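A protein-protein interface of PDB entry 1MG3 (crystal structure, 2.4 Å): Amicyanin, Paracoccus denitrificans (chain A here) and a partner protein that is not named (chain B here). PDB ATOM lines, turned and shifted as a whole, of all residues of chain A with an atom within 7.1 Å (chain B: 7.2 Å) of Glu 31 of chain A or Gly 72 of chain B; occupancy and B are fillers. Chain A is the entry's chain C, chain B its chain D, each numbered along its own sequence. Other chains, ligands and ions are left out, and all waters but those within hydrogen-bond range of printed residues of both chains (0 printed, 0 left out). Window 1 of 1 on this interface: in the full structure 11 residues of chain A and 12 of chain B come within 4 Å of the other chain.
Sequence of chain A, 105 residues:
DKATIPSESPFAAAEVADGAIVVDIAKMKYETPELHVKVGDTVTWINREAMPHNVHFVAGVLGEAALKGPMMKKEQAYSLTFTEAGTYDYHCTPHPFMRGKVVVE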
ATOM      1  N   VAL A  23      -3.695 -14.960  12.202  1.00  0.00           N
ATOM      2  CA  VAL A  23      -4.588 -13.810  12.283  1.00  0.00           C
ATOM      3  C   VAL A  23      -4.896 -13.387  10.852  1.00  0.00           C
ATOM      4  O   VAL A  23      -4.175 -12.578  10.279  1.00  0.00           O
ATOM      5  CB  VAL A  23      -3.932 -12.625  13.032  1.00  0.00           C
ATOM      6  CG1 VAL A  23      -4.747 -11.355  12.833  1.00  0.00           C
ATOM      7  CG2 VAL A  23      -3.839 -12.937  14.509  1.00  0.00           C
ATOM      8  N   ASP A  24      -5.953 -13.950  10.273  1.00  0.00           N
ATOM      9  CA  ASP A  24      -6.341 -13.630   8.897  1.00  0.00           C
ATOM     10  C   ASP A  24      -6.650 -12.149   8.726  1.00  0.00           C
ATOM     11  O   ASP A  24      -7.011 -11.461   9.684  1.00  0.00           O
ATOM     12  CB  ASP A  24      -7.572 -14.439   8.475  1.00  0.00           C
ATOM     13  CG  ASP A  24      -7.300 -15.925   8.406  1.00  0.00           C
ATOM     14  OD1 ASP A  24      -6.490 -16.344   7.555  1.00  0.00           O
ATOM     15  OD2 ASP A  24      -7.898 -16.678   9.203  1.00  0.00           O
ATOM     16  N   ILE A  25      -6.501 -11.664   7.499  1.00  0.00           N
ATOM     17  CA  ILE A  25      -6.779 -10.269   7.189  1.00  0.00           C
ATOM     18  C   ILE A  25      -7.724 -10.246   6.008  1.00  0.00           C
ATOM     19  O   ILE A  25      -7.469 -10.894   4.995  1.00  0.00           O
ATOM     20  CB  ILE A  25      -5.510  -9.504   6.784  1.00  0.00           C
ATOM     21  CG1 ILE A  25      -4.450  -9.617   7.879  1.00  0.00           C
ATOM     22  CG2 ILE A  25      -5.854  -8.049   6.529  1.00  0.00           C
ATOM     23  CD1 ILE A  25      -3.120  -8.976   7.518  1.00  0.00           C
ATOM     24  N   ALA A  26      -8.815  -9.505   6.136  1.00  0.00           N
ATOM     25  CA  ALA A  26      -9.781  -9.416   5.056  1.00  0.00           C
ATOM     26  C   ALA A  26     -10.804  -8.326   5.338  1.00  0.00           C
ATOM     27  O   ALA A  26     -10.897  -7.834   6.459  1.00  0.00           O
ATOM     28  CB  ALA A  26     -10.473 -10.751   4.872  1.00  0.00           C
ATOM     29  N   LYS A  27     -11.561  -7.949   4.312  1.00  0.00           N
ATOM     30  CA  LYS A  27     -12.576  -6.917   4.453  1.00  0.00           C
ATOM     31  C   LYS A  27     -12.053  -5.721   5.237  1.00  0.00           C
ATOM     32  O   LYS A  27     -12.723  -5.202   6.131  1.00  0.00           O
ATOM     33  CB  LYS A  27     -13.821  -7.491   5.139  1.00  0.00           C
ATOM     34  CG  LYS A  27     -14.566  -8.498   4.286  1.00  0.00           C
ATOM     35  CD  LYS A  27     -14.854  -7.909   2.910  1.00  0.00           C
ATOM     36  CE  LYS A  27     -15.418  -8.947   1.960  1.00  0.00           C
ATOM     37  NZ  LYS A  27     -15.665  -8.380   0.608  1.00  0.00           N
ATOM     38  N   MET A  28     -10.845  -5.295   4.895  1.00  0.00           N
ATOM     39  CA  MET A  28     -10.221  -4.158   5.549  1.00  0.00           C
ATOM     40  C   MET A  28     -10.088  -4.305   7.062  1.00  0.00           C
ATOM     41  O   MET A  28     -10.401  -3.366   7.792  1.00  0.00           O
ATOM     42  CB  MET A  28     -11.014  -2.878   5.254  1.00  0.00           C
ATOM     43  CG  MET A  28     -11.203  -2.568   3.775  1.00  0.00           C
ATOM     44  SD  MET A  28      -9.648  -2.297   2.912  1.00  0.00           S
ATOM     45  CE  MET A  28      -9.196  -0.693   3.540  1.00  0.00           C
ATOM     46  N   LYS A  29      -9.642  -5.458   7.555  1.00  0.00           N
ATOM     47  CA  LYS A  29      -9.484  -5.594   9.000  1.00  0.00           C
ATOM     48  C   LYS A  29      -8.809  -6.853   9.505  1.00  0.00           C
ATOM     49  O   LYS A  29      -8.898  -7.919   8.891  1.00  0.00           O
ATOM     50  CB  LYS A  29     -10.838  -5.443   9.714  1.00  0.00           C
ATOM     51  CG  LYS A  29     -11.862  -6.552   9.471  1.00  0.00           C
ATOM     52  CD  LYS A  29     -13.221  -6.126  10.035  1.00  0.00           C
ATOM     53  CE  LYS A  29     -14.349  -7.062   9.622  1.00  0.00           C
ATOM     54  NZ  LYS A  29     -14.278  -8.378  10.311  1.00  0.00           N
ATOM     55  N   TYR A  30      -8.125  -6.707  10.635  1.00  0.00           N
ATOM     56  CA  TYR A  30      -7.448  -7.819  11.276  1.00  0.00           C
ATOM     57  C   TYR A  30      -8.535  -8.593  12.014  1.00  0.00           C
ATOM     58  O   TYR A  30      -8.863  -8.278  13.158  1.00  0.00           O
ATOM     59  CB  TYR A  30      -6.395  -7.312  12.266  1.00  0.00           C
ATOM     60  CG  TYR A  30      -5.318  -6.458  11.632  1.00  0.00           C
ATOM     61  CD1 TYR A  30      -4.611  -6.908  10.516  1.00  0.00           C
ATOM     62  CD2 TYR A  30      -5.000  -5.205  12.148  1.00  0.00           C
ATOM     63  CE1 TYR A  30      -3.612  -6.131   9.927  1.00  0.00           C
ATOM     64  CE2 TYR A  30      -4.003  -4.416  11.565  1.00  0.00           C
ATOM     65  CZ  TYR A  30      -3.315  -4.888  10.456  1.00  0.00           C
ATOM     66  OH  TYR A  30      -2.340  -4.119   9.873  1.00  0.00           O
ATOM     67  N   GLU A  31      -9.094  -9.592  11.331  1.00  0.00           N
ATOM     68  CA  GLU A  31     -10.166 -10.436  11.856  1.00  0.00           C
ATOM     69  C   GLU A  31     -10.046 -10.762  13.347  1.00  0.00           C
ATOM     70  O   GLU A  31     -11.051 -10.980  14.024  1.00  0.00           O
ATOM     71  CB  GLU A  31     -10.246 -11.732  11.045  1.00  0.00           C
ATOM     72  CG  GLU A  31     -10.569 -11.534   9.566  1.00  0.00           C
ATOM     73  CD  GLU A  31     -11.999 -11.067   9.325  1.00  0.00           C
ATOM     74  OE1 GLU A  31     -12.364 -10.840   8.152  1.00  0.00           O
ATOM     75  OE2 GLU A  31     -12.759 -10.930  10.304  1.00  0.00           O
ATOM     76  N   THR A  32      -8.822 -10.803  13.859  1.00  0.00           N
ATOM     77  CA  THR A  32      -8.605 -11.079  15.273  1.00  0.00           C
ATOM     78  C   THR A  32      -7.823  -9.902  15.863  1.00  0.00           C
ATOM     79  O   THR A  32      -6.600  -9.935  15.971  1.00  0.00           O
ATOM     80  CB  THR A  32      -7.834 -12.399  15.462  1.00  0.00           C
ATOM     81  OG1 THR A  32      -8.453 -13.428  14.676  1.00  0.00           O
ATOM     82  CG2 THR A  32      -7.866 -12.823  16.922  1.00  0.00           C
ATOM     83  N   PRO A  33      -8.541  -8.837  16.249  1.00  0.00           N
ATOM     84  CA  PRO A  33      -8.038  -7.587  16.830  1.00  0.00           C
ATOM     85  C   PRO A  33      -7.293  -7.630  18.162  1.00  0.00           C
ATOM     86  O   PRO A  33      -6.386  -6.832  18.388  1.00  0.00           O
ATOM     87  CB  PRO A  33      -9.295  -6.729  16.919  1.00  0.00           C
ATOM     88  CG  PRO A  33     -10.352  -7.736  17.209  1.00  0.00           C
ATOM     89  CD  PRO A  33     -10.015  -8.828  16.217  1.00  0.00           C
ATOM     90  N   GLU A  34      -7.679  -8.529  19.058  1.00  0.00           N
ATOM     91  CA  GLU A  34      -7.007  -8.599  20.348  1.00  0.00           C
ATOM     92  C   GLU A  34      -6.459  -9.999  20.612  1.00  0.00           C
ATOM     93  O   GLU A  34      -6.844 -10.658  21.583  1.00  0.00           O
ATOM     94  CB  GLU A  34      -7.966  -8.188  21.468  1.00  0.00           C
ATOM     95  CG  GLU A  34      -7.271  -7.842  22.781  1.00  0.00           C
ATOM     96  CD  GLU A  34      -8.240  -7.380  23.858  1.00  0.00           C
ATOM     97  OE1 GLU A  34      -9.064  -6.483  23.577  1.00  0.00           O
ATOM     98  OE2 GLU A  34      -8.173  -7.908  24.988  1.00  0.00           O
ATOM     99  N   ARG A  48      -6.133 -12.372   2.960  1.00  0.00           N
ATOM    100  CA  ARG A  48      -7.108 -13.155   2.221  1.00  0.00           C
ATOM    101  C   ARG A  48      -7.795 -12.395   1.096  1.00  0.00           C
ATOM    102  O   ARG A  48      -8.612 -12.964   0.374  1.00  0.00           O
ATOM    103  CB  ARG A  48      -8.161 -13.694   3.186  1.00  0.00           C
ATOM    104  CG  ARG A  48      -7.576 -14.449   4.367  1.00  0.00           C
ATOM    105  CD  ARG A  48      -6.776 -15.668   3.911  1.00  0.00           C
ATOM    106  NE  ARG A  48      -6.331 -16.478   5.042  1.00  0.00           N
ATOM    107  CZ  ARG A  48      -5.807 -17.694   4.933  1.00  0.00           C
ATOM    108  NH1 ARG A  48      -5.432 -18.355   6.019  1.00  0.00           N
ATOM    109  NH2 ARG A  48      -5.662 -18.253   3.740  1.00  0.00           N
ATOM    110  N   TYR A  90      -0.303  -2.603  16.891  1.00  0.00           N
ATOM    111  CA  TYR A  90       0.190  -2.406  15.532  1.00  0.00           C
ATOM    112  C   TYR A  90      -0.919  -1.863  14.637  1.00  0.00           C
ATOM    113  O   TYR A  90      -2.054  -1.679  15.083  1.00  0.00           O
ATOM    114  CB  TYR A  90       0.713  -3.721  14.944  1.00  0.00           C
ATOM    115  CG  TYR A  90      -0.340  -4.800  14.754  1.00  0.00           C
ATOM    116  CD1 TYR A  90      -0.836  -5.527  15.840  1.00  0.00           C
ATOM    117  CD2 TYR A  90      -0.833  -5.103  13.482  1.00  0.00           C
ATOM    118  CE1 TYR A  90      -1.794  -6.531  15.660  1.00  0.00           C
ATOM    119  CE2 TYR A  90      -1.790  -6.101  13.295  1.00  0.00           C
ATOM    120  CZ  TYR A  90      -2.266  -6.808  14.388  1.00  0.00           C
ATOM    121  OH  TYR A  90      -3.222  -7.782  14.207  1.00  0.00           O
ATOM    122  N   ARG A  99      -6.513  -1.290  12.917  1.00  0.00           N
ATOM    123  CA  ARG A  99      -5.728  -1.529  14.110  1.00  0.00           C
ATOM    124  C   ARG A  99      -5.738  -2.982  14.540  1.00  0.00           C
ATOM    125  O   ARG A  99      -6.623  -3.755  14.174  1.00  0.00           O
ATOM    126  CB  ARG A  99      -6.227  -0.672  15.266  1.00  0.00           C
ATOM    127  CG  ARG A  99      -5.197   0.304  15.790  1.00  0.00           C
ATOM    128  CD  ARG A  99      -5.257   1.598  15.014  1.00  0.00           C
ATOM    129  NE  ARG A  99      -6.634   2.087  14.940  1.00  0.00           N
ATOM    130  CZ  ARG A  99      -6.974   3.317  14.571  1.00  0.00           C
ATOM    131  NH1 ARG A  99      -8.255   3.660  14.531  1.00  0.00           N
ATOM    132  NH2 ARG A  99      -6.037   4.206  14.253  1.00  0.00           N
ATOM    133  N   CYS B  60     -15.295 -14.734  23.290  1.00  0.00           N
ATOM    134  CA  CYS B  60     -14.169 -14.886  22.391  1.00  0.00           C
ATOM    135  C   CYS B  60     -14.350 -14.106  21.088  1.00  0.00           C
ATOM    136  O   CYS B  60     -13.398 -13.517  20.584  1.00  0.00           O
ATOM    137  CB  CYS B  60     -13.940 -16.367  22.075  1.00  0.00           C
ATOM    138  SG  CYS B  60     -13.481 -17.441  23.483  1.00  0.00           S
ATOM    139  N   HIS B  61     -15.568 -14.077  20.555  1.00  0.00           N
ATOM    140  CA  HIS B  61     -15.812 -13.395  19.285  1.00  0.00           C
ATOM    141  C   HIS B  61     -16.188 -11.917  19.304  1.00  0.00           C
ATOM    142  O   HIS B  61     -16.334 -11.304  18.246  1.00  0.00           O
ATOM    143  CB  HIS B  61     -16.846 -14.184  18.468  1.00  0.00           C
ATOM    144  CG  HIS B  61     -16.306 -15.464  17.910  1.00  0.00           C
ATOM    145  ND1 HIS B  61     -15.231 -15.459  17.072  1.00  0.00           N
ATOM    146  CD2 HIS B  61     -16.872 -16.634  18.278  1.00  0.00           C
ATOM    147  CE1 HIS B  61     -15.062 -16.812  16.868  1.00  0.00           C
ATOM    148  NE2 HIS B  61     -16.060 -17.554  17.599  1.00  0.00           N
ATOM    149  N   ALA B  65     -19.595  -9.606  17.321  1.00  0.00           N
ATOM    150  CA  ALA B  65     -19.038 -10.569  16.377  1.00  0.00           C
ATOM    151  C   ALA B  65     -17.966  -9.922  15.524  1.00  0.00           C
ATOM    152  O   ALA B  65     -17.601 -10.448  14.477  1.00  0.00           O
ATOM    153  CB  ALA B  65     -20.128 -11.134  15.493  1.00  0.00           C
ATOM    154  N   GLU B  66     -17.467  -8.775  15.979  1.00  0.00           N
ATOM    155  CA  GLU B  66     -16.427  -8.047  15.265  1.00  0.00           C
ATOM    156  C   GLU B  66     -15.077  -8.750  15.436  1.00  0.00           C
ATOM    157  O   GLU B  66     -14.179  -8.600  14.609  1.00  0.00           O
ATOM    158  CB  GLU B  66     -16.321  -6.605  15.786  1.00  0.00           C
ATOM    159  CG  GLU B  66     -15.714  -6.473  17.181  1.00  0.00           C
ATOM    160  CD  GLU B  66     -16.743  -6.559  18.293  1.00  0.00           C
ATOM    161  OE1 GLU B  66     -17.665  -7.394  18.189  1.00  0.00           O
ATOM    162  OE2 GLU B  66     -16.621  -5.799  19.280  1.00  0.00           O
ATOM    163  N   GLY B  67     -14.945  -9.519  16.512  1.00  0.00           N
ATOM    164  CA  GLY B  67     -13.701 -10.219  16.773  1.00  0.00           C
ATOM    165  C   GLY B  67     -13.041  -9.672  18.024  1.00  0.00           C
ATOM    166  O   GLY B  67     -13.257  -8.517  18.394  1.00  0.00           O
ATOM    167  N   LYS B  68     -12.246 -10.505  18.682  1.00  0.00           N
ATOM    168  CA  LYS B  68     -11.540 -10.112  19.905  1.00  0.00           C
ATOM    169  C   LYS B  68     -10.477 -11.177  20.173  1.00  0.00           C
ATOM    170  O   LYS B  68      -9.433 -11.195  19.517  1.00  0.00           O
ATOM    171  CB  LYS B  68     -12.515 -10.022  21.094  1.00  0.00           C
ATOM    172  CG  LYS B  68     -11.837  -9.688  22.427  1.00  0.00           C
ATOM    173  CD  LYS B  68     -12.771  -9.819  23.634  1.00  0.00           C
ATOM    174  CE  LYS B  68     -13.383  -8.491  24.082  1.00  0.00           C
ATOM    175  NZ  LYS B  68     -14.344  -7.923  23.100  1.00  0.00           N
ATOM    176  N   ILE B  69     -10.748 -12.062  21.131  1.00  0.00           N
ATOM    177  CA  ILE B  69      -9.833 -13.153  21.462  1.00  0.00           C
ATOM    178  C   ILE B  69      -9.882 -14.124  20.279  1.00  0.00           C
ATOM    179  O   ILE B  69      -8.937 -14.873  20.021  1.00  0.00           O
ATOM    180  CB  ILE B  69     -10.296 -13.891  22.747  1.00  0.00           C
ATOM    181  CG1 ILE B  69     -10.450 -12.883  23.884  1.00  0.00           C
ATOM    182  CG2 ILE B  69      -9.313 -14.989  23.129  1.00  0.00           C
ATOM    183  CD1 ILE B  69      -9.234 -12.035  24.114  1.00  0.00           C
ATOM    184  N   GLY B  70     -11.002 -14.087  19.562  1.00  0.00           N
ATOM    185  CA  GLY B  70     -11.187 -14.947  18.412  1.00  0.00           C
ATOM    186  C   GLY B  70     -11.490 -14.135  17.172  1.00  0.00           C
ATOM    187  O   GLY B  70     -11.615 -12.907  17.237  1.00  0.00           O
ATOM    188  N   PRO B  71     -11.640 -14.804  16.020  1.00  0.00           N
ATOM    189  CA  PRO B  71     -11.929 -14.186  14.722  1.00  0.00           C
ATOM    190  C   PRO B  71     -13.281 -13.486  14.612  1.00  0.00           C
ATOM    191  O   PRO B  71     -14.158 -13.652  15.460  1.00  0.00           O
ATOM    192  CB  PRO B  71     -11.799 -15.360  13.756  1.00  0.00           C
ATOM    193  CG  PRO B  71     -12.307 -16.501  14.568  1.00  0.00           C
ATOM    194  CD  PRO B  71     -11.647 -16.275  15.913  1.00  0.00           C
ATOM    195  N   GLY B  72     -13.439 -12.697  13.555  1.00  0.00           N
ATOM    196  CA  GLY B  72     -14.683 -11.982  13.340  1.00  0.00           C
ATOM    197  C   GLY B  72     -15.678 -12.876  12.636  1.00  0.00           C
ATOM    198  O   GLY B  72     -15.286 -13.735  11.849  1.00  0.00           O
ATOM    199  N   LEU B  73     -16.961 -12.680  12.923  1.00  0.00           N
ATOM    200  CA  LEU B  73     -18.026 -13.477  12.316  1.00  0.00           C
ATOM    201  C   LEU B  73     -19.068 -12.588  11.660  1.00  0.00           C
ATOM    202  O   LEU B  73     -20.119 -13.072  11.236  1.00  0.00           O
ATOM    203  CB  LEU B  73     -18.723 -14.330  13.382  1.00  0.00           C
ATOM    204  CG  LEU B  73     -18.095 -15.625  13.909  1.00  0.00           C
ATOM    205  CD1 LEU B  73     -16.601 -15.483  14.098  1.00  0.00           C
ATOM    206  CD2 LEU B  73     -18.763 -15.982  15.223  1.00  0.00           C
ATOM    207  N   ASN B  74     -18.781 -11.290  11.571  1.00  0.00           N
ATOM    208  CA  ASN B  74     -19.745 -10.353  11.003  1.00  0.00           C
ATOM    209  C   ASN B  74     -19.442  -9.795   9.618  1.00  0.00           C
ATOM    210  O   ASN B  74     -19.852  -8.682   9.295  1.00  0.00           O
ATOM    211  CB  ASN B  74     -19.981  -9.191  11.978  1.00  0.00           C
ATOM    212  CG  ASN B  74     -18.819  -8.208  12.030  1.00  0.00           C
ATOM    213  OD1 ASN B  74     -17.795  -8.388  11.364  1.00  0.00           O
ATOM    214  ND2 ASN B  74     -18.982  -7.154  12.826  1.00  0.00           N
ATOM    215  N   ASP B  75     -18.741 -10.564   8.795  1.00  0.00           N
ATOM    216  CA  ASP B  75     -18.433 -10.105   7.449  1.00  0.00           C
ATOM    217  C   ASP B  75     -18.414 -11.253   6.442  1.00  0.00           C
ATOM    218  O   ASP B  75     -18.520 -12.424   6.820  1.00  0.00           O
ATOM    219  CB  ASP B  75     -17.104  -9.324   7.440  1.00  0.00           C
ATOM    220  CG  ASP B  75     -15.881 -10.212   7.608  1.00  0.00           C
ATOM    221  OD1 ASP B  75     -14.821  -9.669   7.985  1.00  0.00           O
ATOM    222  OD2 ASP B  75     -15.958 -11.432   7.353  1.00  0.00           O
ATOM    223  N   ALA B  76     -18.283 -10.904   5.163  1.00  0.00           N
ATOM    224  CA  ALA B  76     -18.284 -11.879   4.075  1.00  0.00           C
ATOM    225  C   ALA B  76     -17.102 -12.851   4.055  1.00  0.00           C
ATOM    226  O   ALA B  76     -17.129 -13.855   3.338  1.00  0.00           O
ATOM    227  CB  ALA B  76     -18.389 -11.153   2.734  1.00  0.00           C
ATOM    228  N   TYR B  77     -16.056 -12.563   4.823  1.00  0.00           N
ATOM    229  CA  TYR B  77     -14.930 -13.482   4.844  1.00  0.00           C
ATOM    230  C   TYR B  77     -15.141 -14.609   5.844  1.00  0.00           C
ATOM    231  O   TYR B  77     -15.544 -14.376   6.985  1.00  0.00           O
ATOM    232  CB  TYR B  77     -13.622 -12.786   5.204  1.00  0.00           C
ATOM    233  CG  TYR B  77     -12.519 -13.804   5.395  1.00  0.00           C
ATOM    234  CD1 TYR B  77     -12.019 -14.524   4.309  1.00  0.00           C
ATOM    235  CD2 TYR B  77     -12.036 -14.114   6.671  1.00  0.00           C
ATOM    236  CE1 TYR B  77     -11.067 -15.530   4.483  1.00  0.00           C
ATOM    237  CE2 TYR B  77     -11.083 -15.124   6.859  1.00  0.00           C
ATOM    238  CZ  TYR B  77     -10.605 -15.829   5.759  1.00  0.00           C
ATOM    239  OH  TYR B  77      -9.682 -16.840   5.926  1.00  0.00           O
ATOM    240  N   TRP B  78     -14.849 -15.830   5.410  1.00  0.00           N
ATOM    241  CA  TRP B  78     -14.977 -16.997   6.274  1.00  0.00           C
ATOM    242  C   TRP B  78     -13.796 -17.927   6.057  1.00  0.00           C
ATOM    243  O   TRP B  78     -13.540 -18.365   4.935  1.00  0.00           O
ATOM    244  CB  TRP B  78     -16.274 -17.759   5.988  1.00  0.00           C
ATOM    245  CG  TRP B  78     -17.537 -17.004   6.306  1.00  0.00           C
ATOM    246  CD1 TRP B  78     -18.354 -16.361   5.418  1.00  0.00           C
ATOM    247  CD2 TRP B  78     -18.160 -16.865   7.594  1.00  0.00           C
ATOM    248  NE1 TRP B  78     -19.449 -15.842   6.069  1.00  0.00           N
ATOM    249  CE2 TRP B  78     -19.356 -16.135   7.404  1.00  0.00           C
ATOM    250  CE3 TRP B  78     -17.825 -17.290   8.891  1.00  0.00           C
ATOM    251  CZ2 TRP B  78     -20.221 -15.822   8.462  1.00  0.00           C
ATOM    252  CZ3 TRP B  78     -18.689 -16.974   9.947  1.00  0.00           C
ATOM    253  CH2 TRP B  78     -19.872 -16.249   9.721  1.00  0.00           C
ATOM    254  N   THR B  79     -13.069 -18.217   7.131  1.00  0.00           N
ATOM    255  CA  THR B  79     -11.916 -19.108   7.065  1.00  0.00           C
ATOM    256  C   THR B  79     -12.385 -20.454   6.519  1.00  0.00           C
ATOM    257  O   THR B  79     -11.658 -21.148   5.797  1.00  0.00           O
ATOM    258  CB  THR B  79     -11.287 -19.283   8.456  1.00  0.00           C
ATOM    259  OG1 THR B  79     -10.732 -18.027   8.876  1.00  0.00           O
ATOM    260  CG2 THR B  79     -10.192 -20.349   8.433  1.00  0.00           C
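Glu 31 of chain A touches just these residues of chain B: Glu 66, Gly 67, Gly 70, Pro 71, Gly 72, Asp 75 and Tyr 77.
Of chain A, only Glu 31 comes within 4 Å of Gly 72 of chain B.
Of the printed residues of chain B, Ala 26 of chain A touches Tyr 77.
Of the printed residues of chain A, Thr 79 of chain B touches Asp 24.
The nearest printed residue of chain B that does not touch Lys 29 of chain A is Glu 66 of chain B (4.3 Å).
Of the 15 printed residues of chain A, 9 touch a printed residue of chain B.
Hydrophobic or aromatic side chains of chain B within 4 Å of the printed part of chain A: Ile 69, Pro 71, Ala 76 and Tyr 77.
Among the printed residues, 23 pairs touch across the chains.
Among the printed residues, Asp or Glu carboxylates within 4 Å of a Lys or Arg side-chain nitrogen of the other chain: Lys 29 of chain A with Asp 75 of chain B.
The backbone carbonyl oxygen (O) of Lys 68 of chain B is in hydrogen-bond range of the backbone NH (N) of Glu 34 of chain A.
OE1 of Glu 31 of chain A sits close to OD1 of Asp 75 of chain B, at 2.7 Å.
OH of Tyr 77 of chain B sits at hydrogen-bond distance from NE of Arg 48 of chain A.
OG1 of Thr 79 of chain B sits at hydrogen-bond distance from OD2 of Asp 24 of chain A, 3.2 Å away.
The side-chain amino group (NZ) of Lys 29 of chain A lies within salt-bridge range of the side-chain carboxylate (OD1) of Asp 75 of chain B.
O of Glu 31 of chain A is in hydrogen-bond range of N of Gly 72 of chain B (3.0 Å).
O of Ala 65 of chain B sits at hydrogen-bond distance from N of Asn 74 of chain B, 3.2 Å away.
O of His 61 of chain B sits at hydrogen-bond distance from N of Gly 67 of chain B (2.8 Å).
The backbone carbonyl oxygen (O) of Pro 71 of chain B sits at hydrogen-bond distance from a ring nitrogen (ND1) of His 61 of chain B (2.6 Å).
O of Ile 25 of chain A lies within hydrogen-bond range of N of Arg 48 of chain A, 2.8 Å away.
The backbone NH (N) of Glu 31 of chain A sits at hydrogen-bond distance from the backbone carbonyl oxygen (O) of Asp 24 of chain A.
The backbone carbonyl oxygen (O) of Cys 60 of chain B lies within hydrogen-bond range of the backbone NH (N) of Gly 70 of chain B (2.7 Å).
Among the printed residues, pairs that only touch across the chains: Asp 24 of chain A with Tyr 77 of chain B (3.6 Å), Ala 26 of chain A with Tyr 77 of chain B (3.7 Å), Lys 27 of chain A with Asp 75 of chain B (3.7 Å), Lys 27 of chain A with Ala 76 of chain B (3.8 Å), Lys 29 of chain A with Asn 74 of chain B (3.7 Å), Glu 31 of chain A with Glu 66 of chain B (3.97 Å), Glu 31 of chain A with Gly 67 of chain B (3.9 Å), Glu 31 of chain A with Gly 70 of chain B (3.8 Å), Glu 31 of chain A with Pro 71 of chain B (3.4 Å), Glu 31 of chain A with Tyr 77 of chain B (3.6 Å), Thr 32 of chain A with Lys 68 of chain B (3.4 Å), Thr 32 of chain A with Ile 69 of chain B (3.9 Å), Thr 32 of chain A with Gly 70 of chain B (3.8 Å), Thr 32 of chain A with Pro 71 of chain B (3.6 Å), Pro 33 of chain A with Gly 67 of chain B (3.2 Å), Pro 33 of chain A with Lys 68 of chain B (3.7 Å) and Glu 34 of chain A with Ile 69 of chain B (3.7 Å).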
